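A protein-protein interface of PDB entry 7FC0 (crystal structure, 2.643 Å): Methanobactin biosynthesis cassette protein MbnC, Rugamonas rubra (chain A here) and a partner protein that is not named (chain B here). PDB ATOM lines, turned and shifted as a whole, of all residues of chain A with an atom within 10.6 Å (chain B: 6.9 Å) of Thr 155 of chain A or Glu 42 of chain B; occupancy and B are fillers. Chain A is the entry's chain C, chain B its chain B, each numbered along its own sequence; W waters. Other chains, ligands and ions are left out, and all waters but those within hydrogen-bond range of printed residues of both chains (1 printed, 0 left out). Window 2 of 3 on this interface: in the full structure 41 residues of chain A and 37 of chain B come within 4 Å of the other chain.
Among the printed residues, pairs that only touch across the chains: Val 135 of chain A with Gln 37 of chain B (3.4 Å), Lys 152 of chain A with Gln 37 of chain B (3.8 Å), Pro 153 of chain A with Gln 37 of chain B (3.6 Å), Pro 153 of chain A with Val 38 of chain B (3.8 Å), Asn 154 of chain A with Gln 37 of chain B (3.3 Å), Asn 154 of chain A with Val 38 of chain B (3.5 Å), Asn 154 of chain A with Pro 39 of chain B (3.3 Å), Thr 155 of chain A with Val 38 of chain B (3.8 Å), Thr 155 of chain A with Glu 42 of chain B (3.8 Å), Leu 156 of chain A with Phe 35 of chain B (3.5 Å), Leu 156 of chain A with Leu 43 of chain B (3.8 Å), Leu 156 of chain A with Ala 46 of chain B (3.9 Å) and Tyr 186 of chain A with Gln 37 of chain B (3.5 Å).
Water W1 bridges NZ of Lys 152 of chain A and NE2 of Gln 37 of chain B.
Hydrophobic or aromatic side chains of chain B within 4 Å of the printed part of chain A: Phe 35, Val 38, Pro 39, Leu 43 and Ala 46. Printed residues of chain A that touch a printed residue of chain B: Val 135, Lys 152, Pro 153, Asn 154, Thr 155, Leu 156 and Tyr 186. Hydrophobic or aromatic side chains of chain A that line the printed part of chain B: Val 135, Leu 156 and Tyr 186. Along chain A the printed residues that touch a printed residue of chain B span positions 135 to 186.
O of Gly 10 of chain B lies close to O of Leu 156 of chain A (3.0 Å).
The backbone carbonyl oxygen (O) of Val 135 of chain A is in hydrogen-bond range of the backbone NH (N) of Lys 152 of chain A, at 3.0 Å. The side-chain hydroxyl (OH) of Tyr 186 of chain A is in hydrogen-bond range of the backbone carbonyl oxygen (O) of Lys 152 of chain A (2.8 Å). The backbone NH (N) of Ala 157 of chain A lies within hydrogen-bond range of the side-chain hydroxyl (OG1) of Thr 155 of chain A (3.4 Å).
Trp 151 of chain A touches none of the printed residues of chain B. Of the printed residues of chain B, Asn 154 of chain A touches Gln 37 (3.3 Å), Val 38 (3.5 Å) and Pro 39 (3.3 Å). Of chain B, only Val 38 (3.8 Å) and Glu 42 (3.8 Å) come within 4 Å of Thr 155 of chain A. Of the printed residues of chain B, Leu 156 of chain A touches Gly 10 (3.0 Å), Phe 35 (3.5 Å), Leu 43 (3.8 Å) and Ala 46 (3.9 Å). Arg 161 of chain A touches none of the printed residues of chain B. Of the printed residues of chain B, Tyr 186 of chain A touches Gln 37. Of the printed residues of chain A, Gly 10 of chain B touches Leu 156. Printed residues of chain A within 4 Å of Phe 35 of chain B: Leu 156. Of the printed residues of chain A, Val 38 of chain B touches Pro 153, Asn 154 and Thr 155. Of the printed residues of chain A, Pro 39 of chain B touches Asn 154. Ala 44 of chain B touches none of the printed residues of chain A. The nearest printed residue of chain A that does not touch Glu 42 of chain B is Asn 154 of chain A (4.2 Å).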
ATOM      1  N   VAL A 135      -7.051  33.833 -14.172  1.00  0.00           N
ATOM      2  CA  VAL A 135      -6.756  33.043 -15.363  1.00  0.00           C
ATOM      3  C   VAL A 135      -6.905  33.828 -16.658  1.00  0.00           C
ATOM      4  O   VAL A 135      -6.470  33.331 -17.714  1.00  0.00           O
ATOM      5  CB  VAL A 135      -7.625  31.769 -15.419  1.00  0.00           C
ATOM      6  CG1 VAL A 135      -7.384  30.914 -14.193  1.00  0.00           C
ATOM      7  CG2 VAL A 135      -9.086  32.119 -15.523  1.00  0.00           C
ATOM      8  N   TRP A 151      -5.560  34.103 -22.076  1.00  0.00           N
ATOM      9  CA  TRP A 151      -5.915  32.989 -21.199  1.00  0.00           C
ATOM     10  C   TRP A 151      -4.691  32.175 -20.795  1.00  0.00           C
ATOM     11  O   TRP A 151      -3.923  31.722 -21.654  1.00  0.00           O
ATOM     12  CB  TRP A 151      -6.913  32.050 -21.871  1.00  0.00           C
ATOM     13  CG  TRP A 151      -8.218  32.656 -22.280  1.00  0.00           C
ATOM     14  CD1 TRP A 151      -8.580  33.044 -23.533  1.00  0.00           C
ATOM     15  CD2 TRP A 151      -9.361  32.882 -21.447  1.00  0.00           C
ATOM     16  NE1 TRP A 151      -9.868  33.513 -23.531  1.00  0.00           N
ATOM     17  CE2 TRP A 151     -10.369  33.424 -22.260  1.00  0.00           C
ATOM     18  CE3 TRP A 151      -9.627  32.683 -20.091  1.00  0.00           C
ATOM     19  CZ2 TRP A 151     -11.616  33.773 -21.763  1.00  0.00           C
ATOM     20  CZ3 TRP A 151     -10.868  33.030 -19.600  1.00  0.00           C
ATOM     21  CH2 TRP A 151     -11.849  33.560 -20.434  1.00  0.00           C
ATOM     22  N   LYS A 152      -4.552  31.941 -19.497  1.00  0.00           N
ATOM     23  CA  LYS A 152      -3.575  30.985 -19.005  1.00  0.00           C
ATOM     24  C   LYS A 152      -3.972  29.566 -19.411  1.00  0.00           C
ATOM     25  O   LYS A 152      -5.161  29.240 -19.463  1.00  0.00           O
ATOM     26  CB  LYS A 152      -3.478  31.065 -17.485  1.00  0.00           C
ATOM     27  CG  LYS A 152      -2.680  32.252 -16.981  1.00  0.00           C
ATOM     28  CD  LYS A 152      -2.828  32.359 -15.479  1.00  0.00           C
ATOM     29  CE  LYS A 152      -1.989  33.474 -14.913  1.00  0.00           C
ATOM     30  NZ  LYS A 152      -2.284  33.630 -13.459  1.00  0.00           N
ATOM     31  N   PRO A 153      -3.001  28.697 -19.693  1.00  0.00           N
ATOM     32  CA  PRO A 153      -3.337  27.317 -20.085  1.00  0.00           C
ATOM     33  C   PRO A 153      -3.855  26.506 -18.903  1.00  0.00           C
ATOM     34  O   PRO A 153      -3.282  26.533 -17.810  1.00  0.00           O
ATOM     35  CB  PRO A 153      -2.010  26.756 -20.611  1.00  0.00           C
ATOM     36  CG  PRO A 153      -0.947  27.627 -20.049  1.00  0.00           C
ATOM     37  CD  PRO A 153      -1.553  28.949 -19.653  1.00  0.00           C
ATOM     38  N   ASN A 154      -4.961  25.791 -19.124  1.00  0.00           N
ATOM     39  CA  ASN A 154      -5.527  24.922 -18.101  1.00  0.00           C
ATOM     40  C   ASN A 154      -5.492  23.461 -18.501  1.00  0.00           C
ATOM     41  O   ASN A 154      -6.025  22.616 -17.774  1.00  0.00           O
ATOM     42  CB  ASN A 154      -6.967  25.335 -17.752  1.00  0.00           C
ATOM     43  CG  ASN A 154      -7.904  25.239 -18.923  1.00  0.00           C
ATOM     44  OD1 ASN A 154      -7.482  25.196 -20.079  1.00  0.00           O
ATOM     45  ND2 ASN A 154      -9.193  25.193 -18.630  1.00  0.00           N
ATOM     46  N   THR A 155      -4.894  23.138 -19.636  1.00  0.00           N
ATOM     47  CA  THR A 155      -4.602  21.767 -20.020  1.00  0.00           C
ATOM     48  C   THR A 155      -3.152  21.715 -20.488  1.00  0.00           C
ATOM     49  O   THR A 155      -2.455  22.730 -20.512  1.00  0.00           O
ATOM     50  CB  THR A 155      -5.576  21.263 -21.097  1.00  0.00           C
ATOM     51  OG1 THR A 155      -5.240  21.821 -22.377  1.00  0.00           O
ATOM     52  CG2 THR A 155      -7.006  21.635 -20.734  1.00  0.00           C
ATOM     53  N   LEU A 156      -2.663  20.529 -20.821  1.00  0.00           N
ATOM     54  CA  LEU A 156      -1.329  20.445 -21.392  1.00  0.00           C
ATOM     55  C   LEU A 156      -1.331  20.282 -22.899  1.00  0.00           C
ATOM     56  O   LEU A 156      -0.258  20.182 -23.501  1.00  0.00           O
ATOM     57  CB  LEU A 156      -0.565  19.285 -20.780  1.00  0.00           C
ATOM     58  CG  LEU A 156      -0.628  19.235 -19.279  1.00  0.00           C
ATOM     59  CD1 LEU A 156      -0.348  17.820 -18.789  1.00  0.00           C
ATOM     60  CD2 LEU A 156       0.385  20.254 -18.801  1.00  0.00           C
ATOM     61  N   ALA A 157      -2.499  20.276 -23.527  1.00  0.00           N
ATOM     62  CA  ALA A 157      -2.520  20.171 -24.975  1.00  0.00           C
ATOM     63  C   ALA A 157      -2.135  21.491 -25.628  1.00  0.00           C
ATOM     64  O   ALA A 157      -1.536  21.500 -26.706  1.00  0.00           O
ATOM     65  CB  ALA A 157      -3.893  19.681 -25.439  1.00  0.00           C
ATOM     66  N   ALA A 158      -2.445  22.614 -24.995  1.00  0.00           N
ATOM     67  CA  ALA A 158      -2.123  23.898 -25.585  1.00  0.00           C
ATOM     68  C   ALA A 158      -1.606  24.823 -24.501  1.00  0.00           C
ATOM     69  O   ALA A 158      -1.893  24.650 -23.312  1.00  0.00           O
ATOM     70  CB  ALA A 158      -3.336  24.523 -26.292  1.00  0.00           C
ATOM     71  N   GLY A 159      -0.827  25.806 -24.941  1.00  0.00           N
ATOM     72  CA  GLY A 159      -0.316  26.858 -24.091  1.00  0.00           C
ATOM     73  C   GLY A 159      -1.322  27.972 -23.984  1.00  0.00           C
ATOM     74  O   GLY A 159      -2.533  27.757 -24.136  1.00  0.00           O
ATOM     75  N   ARG A 160      -0.818  29.182 -23.732  1.00  0.00           N
ATOM     76  CA  ARG A 160      -1.705  30.323 -23.595  1.00  0.00           C
ATOM     77  C   ARG A 160      -2.405  30.632 -24.916  1.00  0.00           C
ATOM     78  O   ARG A 160      -1.825  30.506 -25.999  1.00  0.00           O
ATOM     79  CB  ARG A 160      -0.938  31.546 -23.085  1.00  0.00           C
ATOM     80  CG  ARG A 160       0.494  31.748 -23.606  1.00  0.00           C
ATOM     81  CD  ARG A 160       0.577  31.794 -25.073  1.00  0.00           C
ATOM     82  NE  ARG A 160       1.717  32.524 -25.596  1.00  0.00           N
ATOM     83  CZ  ARG A 160       1.888  32.706 -26.900  1.00  0.00           C
ATOM     84  NH1 ARG A 160       0.997  32.209 -27.743  1.00  0.00           N
ATOM     85  NH2 ARG A 160       2.930  33.377 -27.365  1.00  0.00           N
ATOM     86  N   ARG A 161      -3.668  31.031 -24.816  1.00  0.00           N
ATOM     87  CA  ARG A 161      -4.496  31.328 -25.972  1.00  0.00           C
ATOM     88  C   ARG A 161      -4.925  32.770 -25.822  1.00  0.00           C
ATOM     89  O   ARG A 161      -5.395  33.172 -24.755  1.00  0.00           O
ATOM     90  CB  ARG A 161      -5.736  30.415 -26.073  1.00  0.00           C
ATOM     91  CG  ARG A 161      -5.661  29.356 -27.190  1.00  0.00           C
ATOM     92  CD  ARG A 161      -6.904  28.461 -27.281  1.00  0.00           C
ATOM     93  NE  ARG A 161      -7.906  28.948 -28.230  1.00  0.00           N
ATOM     94  CZ  ARG A 161      -8.980  29.659 -27.889  1.00  0.00           C
ATOM     95  NH1 ARG A 161      -9.152  30.041 -26.628  1.00  0.00           N
ATOM     96  NH2 ARG A 161      -9.845  30.050 -28.823  1.00  0.00           N
ATOM     97  N   TYR A 186     -12.681  30.470 -16.109  1.00  0.00           N
ATOM     98  CA  TYR A 186     -12.748  30.337 -17.565  1.00  0.00           C
ATOM     99  C   TYR A 186     -14.155  30.547 -18.072  1.00  0.00           C
ATOM    100  O   TYR A 186     -14.662  29.852 -18.956  1.00  0.00           O
ATOM    101  CB  TYR A 186     -12.207  28.986 -17.987  1.00  0.00           C
ATOM    102  CG  TYR A 186     -10.725  28.894 -17.771  1.00  0.00           C
ATOM    103  CD1 TYR A 186      -9.843  29.375 -18.722  1.00  0.00           C
ATOM    104  CD2 TYR A 186     -10.206  28.344 -16.606  1.00  0.00           C
ATOM    105  CE1 TYR A 186      -8.488  29.299 -18.527  1.00  0.00           C
ATOM    106  CE2 TYR A 186      -8.852  28.268 -16.400  1.00  0.00           C
ATOM    107  CZ  TYR A 186      -7.998  28.739 -17.369  1.00  0.00           C
ATOM    108  OH  TYR A 186      -6.643  28.659 -17.177  1.00  0.00           O
ATOM    109  N   GLY B  10       3.624  22.415 -22.091  1.00  0.00           N
ATOM    110  CA  GLY B  10       2.721  21.296 -22.305  1.00  0.00           C
ATOM    111  C   GLY B  10       2.859  20.650 -23.672  1.00  0.00           C
ATOM    112  O   GLY B  10       2.662  19.438 -23.819  1.00  0.00           O
ATOM    113  N   PHE B  35       2.009  25.514 -14.466  1.00  0.00           N
ATOM    114  CA  PHE B  35       0.831  24.675 -14.662  1.00  0.00           C
ATOM    115  C   PHE B  35      -0.190  24.856 -13.549  1.00  0.00           C
ATOM    116  O   PHE B  35      -1.087  24.024 -13.390  1.00  0.00           O
ATOM    117  CB  PHE B  35       1.237  23.198 -14.794  1.00  0.00           C
ATOM    118  CG  PHE B  35       2.326  22.972 -15.798  1.00  0.00           C
ATOM    119  CD1 PHE B  35       2.023  22.809 -17.137  1.00  0.00           C
ATOM    120  CD2 PHE B  35       3.652  22.982 -15.415  1.00  0.00           C
ATOM    121  CE1 PHE B  35       3.034  22.626 -18.094  1.00  0.00           C
ATOM    122  CE2 PHE B  35       4.663  22.805 -16.360  1.00  0.00           C
ATOM    123  CZ  PHE B  35       4.354  22.626 -17.706  1.00  0.00           C
ATOM    124  N   GLN B  37      -2.816  26.446 -13.324  1.00  0.00           N
ATOM    125  CA  GLN B  37      -4.222  26.432 -13.711  1.00  0.00           C
ATOM    126  C   GLN B  37      -4.623  25.108 -14.348  1.00  0.00           C
ATOM    127  O   GLN B  37      -5.804  24.915 -14.663  1.00  0.00           O
ATOM    128  CB  GLN B  37      -4.539  27.603 -14.652  1.00  0.00           C
ATOM    129  CG  GLN B  37      -3.935  28.952 -14.215  1.00  0.00           C
ATOM    130  CD  GLN B  37      -4.267  29.358 -12.771  1.00  0.00           C
ATOM    131  OE1 GLN B  37      -5.341  29.038 -12.230  1.00  0.00           O
ATOM    132  NE2 GLN B  37      -3.344  30.088 -12.151  1.00  0.00           N
ATOM    133  N   VAL B  38      -3.677  24.193 -14.522  1.00  0.00           N
ATOM    134  CA  VAL B  38      -3.985  22.830 -14.947  1.00  0.00           C
ATOM    135  C   VAL B  38      -4.425  22.038 -13.711  1.00  0.00           C
ATOM    136  O   VAL B  38      -3.675  21.998 -12.727  1.00  0.00           O
ATOM    137  CB  VAL B  38      -2.760  22.193 -15.599  1.00  0.00           C
ATOM    138  CG1 VAL B  38      -3.047  20.777 -16.072  1.00  0.00           C
ATOM    139  CG2 VAL B  38      -2.290  23.056 -16.755  1.00  0.00           C
ATOM    140  N   PRO B  39      -5.596  21.406 -13.730  1.00  0.00           N
ATOM    141  CA  PRO B  39      -6.090  20.697 -12.529  1.00  0.00           C
ATOM    142  C   PRO B  39      -5.067  19.725 -11.981  1.00  0.00           C
ATOM    143  O   PRO B  39      -4.493  18.923 -12.732  1.00  0.00           O
ATOM    144  CB  PRO B  39      -7.334  19.967 -13.042  1.00  0.00           C
ATOM    145  CG  PRO B  39      -7.855  20.915 -14.101  1.00  0.00           C
ATOM    146  CD  PRO B  39      -6.636  21.516 -14.765  1.00  0.00           C
ATOM    147  N   PRO B  40      -4.811  19.783 -10.669  1.00  0.00           N
ATOM    148  CA  PRO B  40      -3.747  18.950 -10.073  1.00  0.00           C
ATOM    149  C   PRO B  40      -3.902  17.467 -10.358  1.00  0.00           C
ATOM    150  O   PRO B  40      -2.910  16.771 -10.603  1.00  0.00           O
ATOM    151  CB  PRO B  40      -3.871  19.256  -8.574  1.00  0.00           C
ATOM    152  CG  PRO B  40      -4.495  20.594  -8.522  1.00  0.00           C
ATOM    153  CD  PRO B  40      -5.448  20.658  -9.675  1.00  0.00           C
ATOM    154  N   GLN B  41      -5.132  16.963 -10.345  1.00  0.00           N
ATOM    155  CA  GLN B  41      -5.323  15.562 -10.665  1.00  0.00           C
ATOM    156  C   GLN B  41      -4.992  15.292 -12.127  1.00  0.00           C
ATOM    157  O   GLN B  41      -4.344  14.294 -12.447  1.00  0.00           O
ATOM    158  CB  GLN B  41      -6.763  15.160 -10.328  1.00  0.00           C
ATOM    159  CG  GLN B  41      -7.003  13.659 -10.221  1.00  0.00           C
ATOM    160  CD  GLN B  41      -5.986  12.954  -9.332  1.00  0.00           C
ATOM    161  OE1 GLN B  41      -5.477  13.527  -8.362  1.00  0.00           O
ATOM    162  NE2 GLN B  41      -5.668  11.704  -9.678  1.00  0.00           N
ATOM    163  N   GLU B  42      -5.353  16.205 -13.020  1.00  0.00           N
ATOM    164  CA  GLU B  42      -5.036  15.995 -14.427  1.00  0.00           C
ATOM    165  C   GLU B  42      -3.533  16.018 -14.670  1.00  0.00           C
ATOM    166  O   GLU B  42      -3.016  15.218 -15.461  1.00  0.00           O
ATOM    167  CB  GLU B  42      -5.737  17.055 -15.281  1.00  0.00           C
ATOM    168  CG  GLU B  42      -5.463  16.925 -16.766  1.00  0.00           C
ATOM    169  CD  GLU B  42      -6.076  18.052 -17.601  1.00  0.00           C
ATOM    170  OE1 GLU B  42      -7.095  18.642 -17.163  1.00  0.00           O
ATOM    171  OE2 GLU B  42      -5.525  18.342 -18.696  1.00  0.00           O
ATOM    172  N   LEU B  43      -2.808  16.897 -13.973  1.00  0.00           N
ATOM    173  CA  LEU B  43      -1.351  16.892 -14.063  1.00  0.00           C
ATOM    174  C   LEU B  43      -0.786  15.550 -13.649  1.00  0.00           C
ATOM    175  O   LEU B  43       0.089  14.998 -14.322  1.00  0.00           O
ATOM    176  CB  LEU B  43      -0.757  17.978 -13.176  1.00  0.00           C
ATOM    177  CG  LEU B  43      -0.345  19.327 -13.753  1.00  0.00           C
ATOM    178  CD1 LEU B  43       0.605  19.985 -12.770  1.00  0.00           C
ATOM    179  CD2 LEU B  43       0.274  19.209 -15.137  1.00  0.00           C
ATOM    180  N   ALA B  44      -1.279  15.011 -12.531  1.00  0.00           N
ATOM    181  CA  ALA B  44      -0.740  13.767 -11.998  1.00  0.00           C
ATOM    182  C   ALA B  44      -0.984  12.583 -12.926  1.00  0.00           C
ATOM    183  O   ALA B  44      -0.147  11.676 -12.998  1.00  0.00           O
ATOM    184  CB  ALA B  44      -1.343  13.485 -10.624  1.00  0.00           C
ATOM    185  N   GLU B  45      -2.081  12.587 -13.675  1.00  0.00           N
ATOM    186  CA  GLU B  45      -2.405  11.462 -14.538  1.00  0.00           C
ATOM    187  C   GLU B  45      -1.683  11.532 -15.870  1.00  0.00           C
ATOM    188  O   GLU B  45      -1.926  10.684 -16.728  1.00  0.00           O
ATOM    189  CB  GLU B  45      -3.921  11.383 -14.788  1.00  0.00           C
ATOM    190  CG  GLU B  45      -4.799  11.495 -13.546  1.00  0.00           C
ATOM    191  CD  GLU B  45      -6.276  11.647 -13.882  1.00  0.00           C
ATOM    192  OE1 GLU B  45      -6.847  12.730 -13.595  1.00  0.00           O
ATOM    193  OE2 GLU B  45      -6.866  10.685 -14.418  1.00  0.00           O
ATOM    194  N   ALA B  46      -0.768  12.486 -16.051  1.00  0.00           N
ATOM    195  CA  ALA B  46      -0.036  12.609 -17.306  1.00  0.00           C
ATOM    196  C   ALA B  46       1.350  11.990 -17.278  1.00  0.00           C
ATOM    197  O   ALA B  46       1.961  11.822 -18.343  1.00  0.00           O
ATOM    198  CB  ALA B  46       0.108  14.083 -17.701  1.00  0.00           C
ATOM    199  N   PHE B  47       1.813  11.721 -16.068  1.00  0.00           N
ATOM    200  CA  PHE B  47       3.185  11.200 -15.921  1.00  0.00           C
ATOM    201  C   PHE B  47       3.169   9.864 -15.190  1.00  0.00           C
ATOM    202  O   PHE B  47       2.748   9.816 -14.035  1.00  0.00           O
ATOM    203  CB  PHE B  47       4.055  12.230 -15.215  1.00  0.00           C
ATOM    204  CG  PHE B  47       4.232  13.533 -15.944  1.00  0.00           C
ATOM    205  CD1 PHE B  47       3.422  14.618 -15.660  1.00  0.00           C
ATOM    206  CD2 PHE B  47       5.220  13.675 -16.901  1.00  0.00           C
ATOM    207  CE1 PHE B  47       3.588  15.815 -16.332  1.00  0.00           C
ATOM    208  CE2 PHE B  47       5.386  14.876 -17.568  1.00  0.00           C
ATOM    209  CZ  PHE B  47       4.569  15.939 -17.282  1.00  0.00           C
ATOM    210  N   LEU B  82       0.764  15.448  -6.706  1.00  0.00           N
ATOM    211  CA  LEU B  82       1.840  14.814  -7.448  1.00  0.00           C
ATOM    212  C   LEU B  82       2.943  14.246  -6.551  1.00  0.00           C
ATOM    213  O   LEU B  82       3.777  13.471  -7.037  1.00  0.00           O
ATOM    214  CB  LEU B  82       2.431  15.827  -8.442  1.00  0.00           C
ATOM    215  CG  LEU B  82       1.625  16.185  -9.690  1.00  0.00           C
ATOM    216  CD1 LEU B  82       0.500  17.110  -9.376  1.00  0.00           C
ATOM    217  CD2 LEU B  82       2.515  16.843 -10.715  1.00  0.00           C
HETATM  218  O   HOH W   1      -0.842  31.404 -12.747  1.00  0.00           O
